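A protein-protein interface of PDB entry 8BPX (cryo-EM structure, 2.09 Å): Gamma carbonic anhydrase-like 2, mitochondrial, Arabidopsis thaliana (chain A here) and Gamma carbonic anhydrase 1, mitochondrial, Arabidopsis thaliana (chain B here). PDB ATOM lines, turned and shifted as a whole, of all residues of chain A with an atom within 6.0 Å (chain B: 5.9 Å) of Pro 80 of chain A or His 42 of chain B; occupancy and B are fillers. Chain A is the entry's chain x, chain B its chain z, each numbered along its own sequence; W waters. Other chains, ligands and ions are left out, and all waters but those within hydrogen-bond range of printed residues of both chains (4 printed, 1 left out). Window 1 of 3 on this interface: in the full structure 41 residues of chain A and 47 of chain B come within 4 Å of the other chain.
The side-chain amide nitrogen of Gln 61 of chain A is in hydrogen-bond range of the backbone carbonyl oxygen of Pro 80 of chain A. The side-chain hydroxyl (OG) of Ser 40 of chain B lies within hydrogen-bond range of the backbone NH (N) of His 42 of chain B. A ring nitrogen (NE2) of His 42 of chain B sits at hydrogen-bond distance from the backbone carbonyl oxygen (O) of Pro 63 of chain B, 2.9 Å away. A ring nitrogen (NE2) of His 42 of chain B sits close to the backbone carbonyl oxygen of Ala 65 of chain B (3.3 Å). The guanidinium group (NH2) of Arg 43 of chain B lies close to the side-chain sulfur (SD) of Met 46 of chain B, 3.6 Å away.
Among the printed residues, merely in contact across the chains: Phe 235 of chain A with Arg 43 of chain B (3.6 Å), Pro 80 of chain A with Arg 41 of chain B (3.6 Å), Asn 81 of chain A with Ser 66 of chain B (3.6 Å), Asn 98 of chain A with Ser 66 of chain B (3.6 Å), Pro 80 of chain A with His 42 of chain B (3.6 Å) and Phe 235 of chain A with Met 46 of chain B (3.8 Å).
Tyr 77 of chain A touches none of the printed residues of chain B. Of chain B, only Arg 41 (3.6 Å) and His 42 (3.6 Å) come within 4 Å of Pro 80 of chain A. Of the printed residues of chain B, Phe 235 of chain A touches Arg 43 and Met 46. Of chain A, only Pro 80 comes within 4 Å of His 42 of chain B. Of the printed residues of chain A, Arg 43 of chain B touches Phe 235 (3.6 Å). Ala 62 of chain B touches none of the printed residues of chain A. The nearest residue of chain B that does not touch Pro 80 of chain A is Ser 40 of chain B (4.8 Å). The nearest residue of chain A that does not touch His 42 of chain B is Asn 81 of chain A (4.1 Å).
Printed residues of chain B that touch a printed residue of chain A: Arg 41, His 42, Arg 43, Met 46 and Ser 66. Of the 10 printed residues of chain A, 4 touch a printed residue of chain B. Hydrophobic or aromatic side chains of chain A within 4 Å of the printed part of chain B: Pro 80 and Phe 235. Among the printed residues, 6 pairs touch across the chains.
Water W2 lies within hydrogen-bond range of ND2 of Asn 98 of chain A (2.6 Å) and SD of Met 46 of chain B (3.1 Å). Water W3 bridges O of Ser 64 of chain B (2.6 Å) and ND2 of Asn 81 of chain A (3.2 Å). Water W4 lies within hydrogen-bond range of O of Pro 80 of chain A and N of Arg 41 of chain B. Water W1 lies within hydrogen-bond range of the backbone NH of Ser 40 of chain B (2.9 Å) and the backbone carbonyl oxygen of Gln 59 of chain A (3.4 Å).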
ATOM      1  N   GLN A  59     -23.231 -12.632 -22.935  1.00  0.00           N
ATOM      2  CA  GLN A  59     -24.234 -11.578 -23.006  1.00  0.00           C
ATOM      3  C   GLN A  59     -24.115 -10.679 -21.782  1.00  0.00           C
ATOM      4  O   GLN A  59     -24.177 -11.162 -20.648  1.00  0.00           O
ATOM      5  CB  GLN A  59     -25.632 -12.184 -23.100  1.00  0.00           C
ATOM      6  CG  GLN A  59     -26.752 -11.185 -22.879  1.00  0.00           C
ATOM      7  CD  GLN A  59     -26.897 -10.205 -24.031  1.00  0.00           C
ATOM      8  OE1 GLN A  59     -27.147 -10.603 -25.164  1.00  0.00           O
ATOM      9  NE2 GLN A  59     -26.740  -8.921 -23.742  1.00  0.00           N
ATOM     10  N   GLN A  61     -25.260  -8.458 -18.868  1.00  0.00           N
ATOM     11  CA  GLN A  61     -26.499  -8.455 -18.098  1.00  0.00           C
ATOM     12  C   GLN A  61     -27.194  -7.098 -18.157  1.00  0.00           C
ATOM     13  O   GLN A  61     -28.425  -7.029 -18.253  1.00  0.00           O
ATOM     14  CB  GLN A  61     -26.217  -8.849 -16.649  1.00  0.00           C
ATOM     15  CG  GLN A  61     -27.451  -8.899 -15.772  1.00  0.00           C
ATOM     16  CD  GLN A  61     -27.139  -9.271 -14.336  1.00  0.00           C
ATOM     17  OE1 GLN A  61     -26.727  -8.430 -13.543  1.00  0.00           O
ATOM     18  NE2 GLN A  61     -27.343 -10.536 -13.995  1.00  0.00           N
ATOM     19  N   TYR A  77     -31.582  -9.547  -5.862  1.00  0.00           N
ATOM     20  CA  TYR A  77     -30.917 -10.634  -6.569  1.00  0.00           C
ATOM     21  C   TYR A  77     -31.339 -10.623  -8.032  1.00  0.00           C
ATOM     22  O   TYR A  77     -32.530 -10.709  -8.340  1.00  0.00           O
ATOM     23  CB  TYR A  77     -31.237 -11.994  -5.952  1.00  0.00           C
ATOM     24  CG  TYR A  77     -30.658 -13.132  -6.759  1.00  0.00           C
ATOM     25  CD1 TYR A  77     -29.287 -13.293  -6.874  1.00  0.00           C
ATOM     26  CD2 TYR A  77     -31.481 -14.027  -7.435  1.00  0.00           C
ATOM     27  CE1 TYR A  77     -28.745 -14.319  -7.617  1.00  0.00           C
ATOM     28  CE2 TYR A  77     -30.945 -15.064  -8.186  1.00  0.00           C
ATOM     29  CZ  TYR A  77     -29.575 -15.198  -8.273  1.00  0.00           C
ATOM     30  OH  TYR A  77     -29.021 -16.215  -9.012  1.00  0.00           O
ATOM     31  N   VAL A  78     -30.365 -10.532  -8.930  1.00  0.00           N
ATOM     32  CA  VAL A  78     -30.596 -10.677 -10.361  1.00  0.00           C
ATOM     33  C   VAL A  78     -29.706 -11.809 -10.854  1.00  0.00           C
ATOM     34  O   VAL A  78     -28.478 -11.736 -10.729  1.00  0.00           O
ATOM     35  CB  VAL A  78     -30.320  -9.373 -11.126  1.00  0.00           C
ATOM     36  CG1 VAL A  78     -30.541  -9.580 -12.614  1.00  0.00           C
ATOM     37  CG2 VAL A  78     -31.210  -8.254 -10.600  1.00  0.00           C
ATOM     38  N   ALA A  79     -30.324 -12.845 -11.415  1.00  0.00           N
ATOM     39  CA  ALA A  79     -29.582 -14.015 -11.856  1.00  0.00           C
ATOM     40  C   ALA A  79     -28.572 -13.624 -12.936  1.00  0.00           C
ATOM     41  O   ALA A  79     -28.797 -12.675 -13.692  1.00  0.00           O
ATOM     42  CB  ALA A  79     -30.535 -15.085 -12.387  1.00  0.00           C
ATOM     43  N   PRO A  80     -27.441 -14.333 -13.016  1.00  0.00           N
ATOM     44  CA  PRO A  80     -26.369 -13.903 -13.935  1.00  0.00           C
ATOM     45  C   PRO A  80     -26.782 -13.811 -15.397  1.00  0.00           C
ATOM     46  O   PRO A  80     -26.297 -12.919 -16.102  1.00  0.00           O
ATOM     47  CB  PRO A  80     -25.287 -14.971 -13.719  1.00  0.00           C
ATOM     48  CG  PRO A  80     -25.551 -15.504 -12.360  1.00  0.00           C
ATOM     49  CD  PRO A  80     -27.040 -15.498 -12.208  1.00  0.00           C
ATOM     50  N   ASN A  81     -27.658 -14.690 -15.881  1.00  0.00           N
ATOM     51  CA  ASN A  81     -27.998 -14.705 -17.299  1.00  0.00           C
ATOM     52  C   ASN A  81     -29.248 -13.889 -17.625  1.00  0.00           C
ATOM     53  O   ASN A  81     -29.718 -13.931 -18.765  1.00  0.00           O
ATOM     54  CB  ASN A  81     -28.149 -16.147 -17.799  1.00  0.00           C
ATOM     55  CG  ASN A  81     -29.365 -16.851 -17.231  1.00  0.00           C
ATOM     56  OD1 ASN A  81     -29.891 -16.475 -16.188  1.00  0.00           O
ATOM     57  ND2 ASN A  81     -29.801 -17.901 -17.911  1.00  0.00           N
ATOM     58  N   VAL A  82     -29.788 -13.151 -16.654  1.00  0.00           N
ATOM     59  CA  VAL A  82     -30.882 -12.225 -16.920  1.00  0.00           C
ATOM     60  C   VAL A  82     -30.378 -11.072 -17.787  1.00  0.00           C
ATOM     61  O   VAL A  82     -29.217 -10.654 -17.691  1.00  0.00           O
ATOM     62  CB  VAL A  82     -31.470 -11.711 -15.591  1.00  0.00           C
ATOM     63  CG1 VAL A  82     -32.433 -10.549 -15.813  1.00  0.00           C
ATOM     64  CG2 VAL A  82     -32.153 -12.838 -14.837  1.00  0.00           C
ATOM     65  N   ASN A  98     -33.321 -16.980 -13.387  1.00  0.00           N
ATOM     66  CA  ASN A  98     -32.593 -17.394 -14.584  1.00  0.00           C
ATOM     67  C   ASN A  98     -33.441 -17.312 -15.847  1.00  0.00           C
ATOM     68  O   ASN A  98     -34.589 -17.758 -15.875  1.00  0.00           O
ATOM     69  CB  ASN A  98     -32.076 -18.827 -14.410  1.00  0.00           C
ATOM     70  CG  ASN A  98     -31.165 -18.982 -13.208  1.00  0.00           C
ATOM     71  OD1 ASN A  98     -31.612 -18.951 -12.068  1.00  0.00           O
ATOM     72  ND2 ASN A  98     -29.879 -19.173 -13.466  1.00  0.00           N
ATOM     73  N   PHE A 235     -22.365 -15.062  -4.677  1.00  0.00           N
ATOM     74  CA  PHE A 235     -21.618 -14.231  -5.614  1.00  0.00           C
ATOM     75  C   PHE A 235     -20.872 -13.140  -4.860  1.00  0.00           C
ATOM     76  O   PHE A 235     -21.488 -12.334  -4.158  1.00  0.00           O
ATOM     77  CB  PHE A 235     -22.552 -13.613  -6.658  1.00  0.00           C
ATOM     78  CG  PHE A 235     -23.197 -14.619  -7.561  1.00  0.00           C
ATOM     79  CD1 PHE A 235     -22.548 -15.065  -8.700  1.00  0.00           C
ATOM     80  CD2 PHE A 235     -24.451 -15.131  -7.266  1.00  0.00           C
ATOM     81  CE1 PHE A 235     -23.139 -15.992  -9.531  1.00  0.00           C
ATOM     82  CE2 PHE A 235     -25.046 -16.062  -8.091  1.00  0.00           C
ATOM     83  CZ  PHE A 235     -24.390 -16.492  -9.227  1.00  0.00           C
ATOM     84  N   SER B  40     -19.807 -12.301 -18.366  1.00  0.00           N
ATOM     85  CA  SER B  40     -20.952 -13.063 -17.888  1.00  0.00           C
ATOM     86  C   SER B  40     -20.551 -13.983 -16.742  1.00  0.00           C
ATOM     87  O   SER B  40     -19.549 -14.697 -16.819  1.00  0.00           O
ATOM     88  CB  SER B  40     -21.559 -13.879 -19.025  1.00  0.00           C
ATOM     89  OG  SER B  40     -22.548 -14.762 -18.531  1.00  0.00           O
ATOM     90  N   ARG B  41     -21.351 -13.971 -15.684  1.00  0.00           N
ATOM     91  CA  ARG B  41     -21.146 -14.836 -14.535  1.00  0.00           C
ATOM     92  C   ARG B  41     -22.017 -16.083 -14.595  1.00  0.00           C
ATOM     93  O   ARG B  41     -22.154 -16.784 -13.590  1.00  0.00           O
ATOM     94  CB  ARG B  41     -21.392 -14.052 -13.247  1.00  0.00           C
ATOM     95  CG  ARG B  41     -20.707 -12.689 -13.259  1.00  0.00           C
ATOM     96  CD  ARG B  41     -20.643 -12.042 -11.887  1.00  0.00           C
ATOM     97  NE  ARG B  41     -19.916 -12.847 -10.913  1.00  0.00           N
ATOM     98  CZ  ARG B  41     -19.591 -12.429  -9.696  1.00  0.00           C
ATOM     99  NH1 ARG B  41     -19.901 -11.213  -9.279  1.00  0.00           N
ATOM    100  NH2 ARG B  41     -18.944 -13.253  -8.877  1.00  0.00           N
ATOM    101  N   HIS B  42     -22.616 -16.361 -15.749  1.00  0.00           N
ATOM    102  CA  HIS B  42     -23.418 -17.562 -15.912  1.00  0.00           C
ATOM    103  C   HIS B  42     -22.561 -18.806 -15.735  1.00  0.00           C
ATOM    104  O   HIS B  42     -21.471 -18.911 -16.298  1.00  0.00           O
ATOM    105  CB  HIS B  42     -24.074 -17.582 -17.291  1.00  0.00           C
ATOM    106  CG  HIS B  42     -24.630 -18.920 -17.666  1.00  0.00           C
ATOM    107  ND1 HIS B  42     -25.780 -19.429 -17.105  1.00  0.00           N
ATOM    108  CD2 HIS B  42     -24.188 -19.860 -18.533  1.00  0.00           C
ATOM    109  CE1 HIS B  42     -26.029 -20.621 -17.616  1.00  0.00           C
ATOM    110  NE2 HIS B  42     -25.075 -20.907 -18.485  1.00  0.00           N
ATOM    111  N   ARG B  43     -23.068 -19.753 -14.956  1.00  0.00           N
ATOM    112  CA  ARG B  43     -22.453 -21.060 -14.795  1.00  0.00           C
ATOM    113  C   ARG B  43     -23.438 -22.113 -15.277  1.00  0.00           C
ATOM    114  O   ARG B  43     -24.592 -22.131 -14.840  1.00  0.00           O
ATOM    115  CB  ARG B  43     -22.062 -21.308 -13.333  1.00  0.00           C
ATOM    116  CG  ARG B  43     -20.748 -20.648 -12.926  1.00  0.00           C
ATOM    117  CD  ARG B  43     -20.480 -20.788 -11.434  1.00  0.00           C
ATOM    118  NE  ARG B  43     -21.446 -20.048 -10.633  1.00  0.00           N
ATOM    119  CZ  ARG B  43     -21.669 -20.252  -9.342  1.00  0.00           C
ATOM    120  NH1 ARG B  43     -20.995 -21.162  -8.656  1.00  0.00           N
ATOM    121  NH2 ARG B  43     -22.581 -19.512  -8.718  1.00  0.00           N
ATOM    122  N   THR B  44     -22.987 -22.975 -16.187  1.00  0.00           N
ATOM    123  CA  THR B  44     -23.854 -24.042 -16.678  1.00  0.00           C
ATOM    124  C   THR B  44     -24.277 -24.962 -15.542  1.00  0.00           C
ATOM    125  O   THR B  44     -25.448 -25.346 -15.445  1.00  0.00           O
ATOM    126  CB  THR B  44     -23.140 -24.830 -17.777  1.00  0.00           C
ATOM    127  OG1 THR B  44     -22.692 -23.932 -18.798  1.00  0.00           O
ATOM    128  CG2 THR B  44     -24.071 -25.854 -18.389  1.00  0.00           C
ATOM    129  N   MET B  46     -24.348 -24.949 -11.398  1.00  0.00           N
ATOM    130  CA  MET B  46     -24.243 -24.048 -10.259  1.00  0.00           C
ATOM    131  C   MET B  46     -24.576 -24.791  -8.979  1.00  0.00           C
ATOM    132  O   MET B  46     -25.608 -25.465  -8.896  1.00  0.00           O
ATOM    133  CB  MET B  46     -25.173 -22.841 -10.412  1.00  0.00           C
ATOM    134  CG  MET B  46     -24.906 -21.750  -9.395  1.00  0.00           C
ATOM    135  SD  MET B  46     -25.959 -20.301  -9.586  1.00  0.00           S
ATOM    136  CE  MET B  46     -26.062 -19.744  -7.885  1.00  0.00           C
ATOM    137  N   ALA B  62     -26.186 -28.136 -22.993  1.00  0.00           N
ATOM    138  CA  ALA B  62     -25.847 -26.943 -23.750  1.00  0.00           C
ATOM    139  C   ALA B  62     -25.236 -25.900 -22.819  1.00  0.00           C
ATOM    140  O   ALA B  62     -25.670 -25.761 -21.671  1.00  0.00           O
ATOM    141  CB  ALA B  62     -27.082 -26.374 -24.449  1.00  0.00           C
ATOM    142  N   PRO B  63     -24.221 -25.160 -23.272  1.00  0.00           N
ATOM    143  CA  PRO B  63     -23.557 -24.197 -22.374  1.00  0.00           C
ATOM    144  C   PRO B  63     -24.498 -23.162 -21.785  1.00  0.00           C
ATOM    145  O   PRO B  63     -24.325 -22.762 -20.627  1.00  0.00           O
ATOM    146  CB  PRO B  63     -22.496 -23.551 -23.278  1.00  0.00           C
ATOM    147  CG  PRO B  63     -22.265 -24.540 -24.370  1.00  0.00           C
ATOM    148  CD  PRO B  63     -23.572 -25.241 -24.591  1.00  0.00           C
ATOM    149  N   SER B  64     -25.500 -22.724 -22.546  1.00  0.00           N
ATOM    150  CA  SER B  64     -26.437 -21.711 -22.081  1.00  0.00           C
ATOM    151  C   SER B  64     -27.485 -22.255 -21.115  1.00  0.00           C
ATOM    152  O   SER B  64     -28.249 -21.465 -20.553  1.00  0.00           O
ATOM    153  CB  SER B  64     -27.131 -21.051 -23.279  1.00  0.00           C
ATOM    154  OG  SER B  64     -27.939 -21.979 -23.984  1.00  0.00           O
ATOM    155  N   ALA B  65     -27.548 -23.568 -20.913  1.00  0.00           N
ATOM    156  CA  ALA B  65     -28.496 -24.131 -19.962  1.00  0.00           C
ATOM    157  C   ALA B  65     -28.081 -23.812 -18.530  1.00  0.00           C
ATOM    158  O   ALA B  65     -26.901 -23.625 -18.227  1.00  0.00           O
ATOM    159  CB  ALA B  65     -28.606 -25.643 -20.149  1.00  0.00           C
ATOM    160  N   SER B  66     -29.070 -23.746 -17.642  1.00  0.00           N
ATOM    161  CA  SER B  66     -28.851 -23.505 -16.222  1.00  0.00           C
ATOM    162  C   SER B  66     -29.248 -24.748 -15.436  1.00  0.00           C
ATOM    163  O   SER B  66     -30.423 -25.129 -15.421  1.00  0.00           O
ATOM    164  CB  SER B  66     -29.645 -22.291 -15.735  1.00  0.00           C
ATOM    165  OG  SER B  66     -29.313 -21.123 -16.458  1.00  0.00           O
HETATM  166  O   HOH W   1     -21.038 -10.118 -19.866  1.00  0.00           O
HETATM  167  O   HOH W   2     -28.164 -20.036 -11.740  1.00  0.00           O
HETATM  168  O   HOH W   3     -27.672 -18.965 -20.071  1.00  0.00           O
HETATM  169  O   HOH W   4     -23.664 -12.103 -15.401  1.00  0.00           O
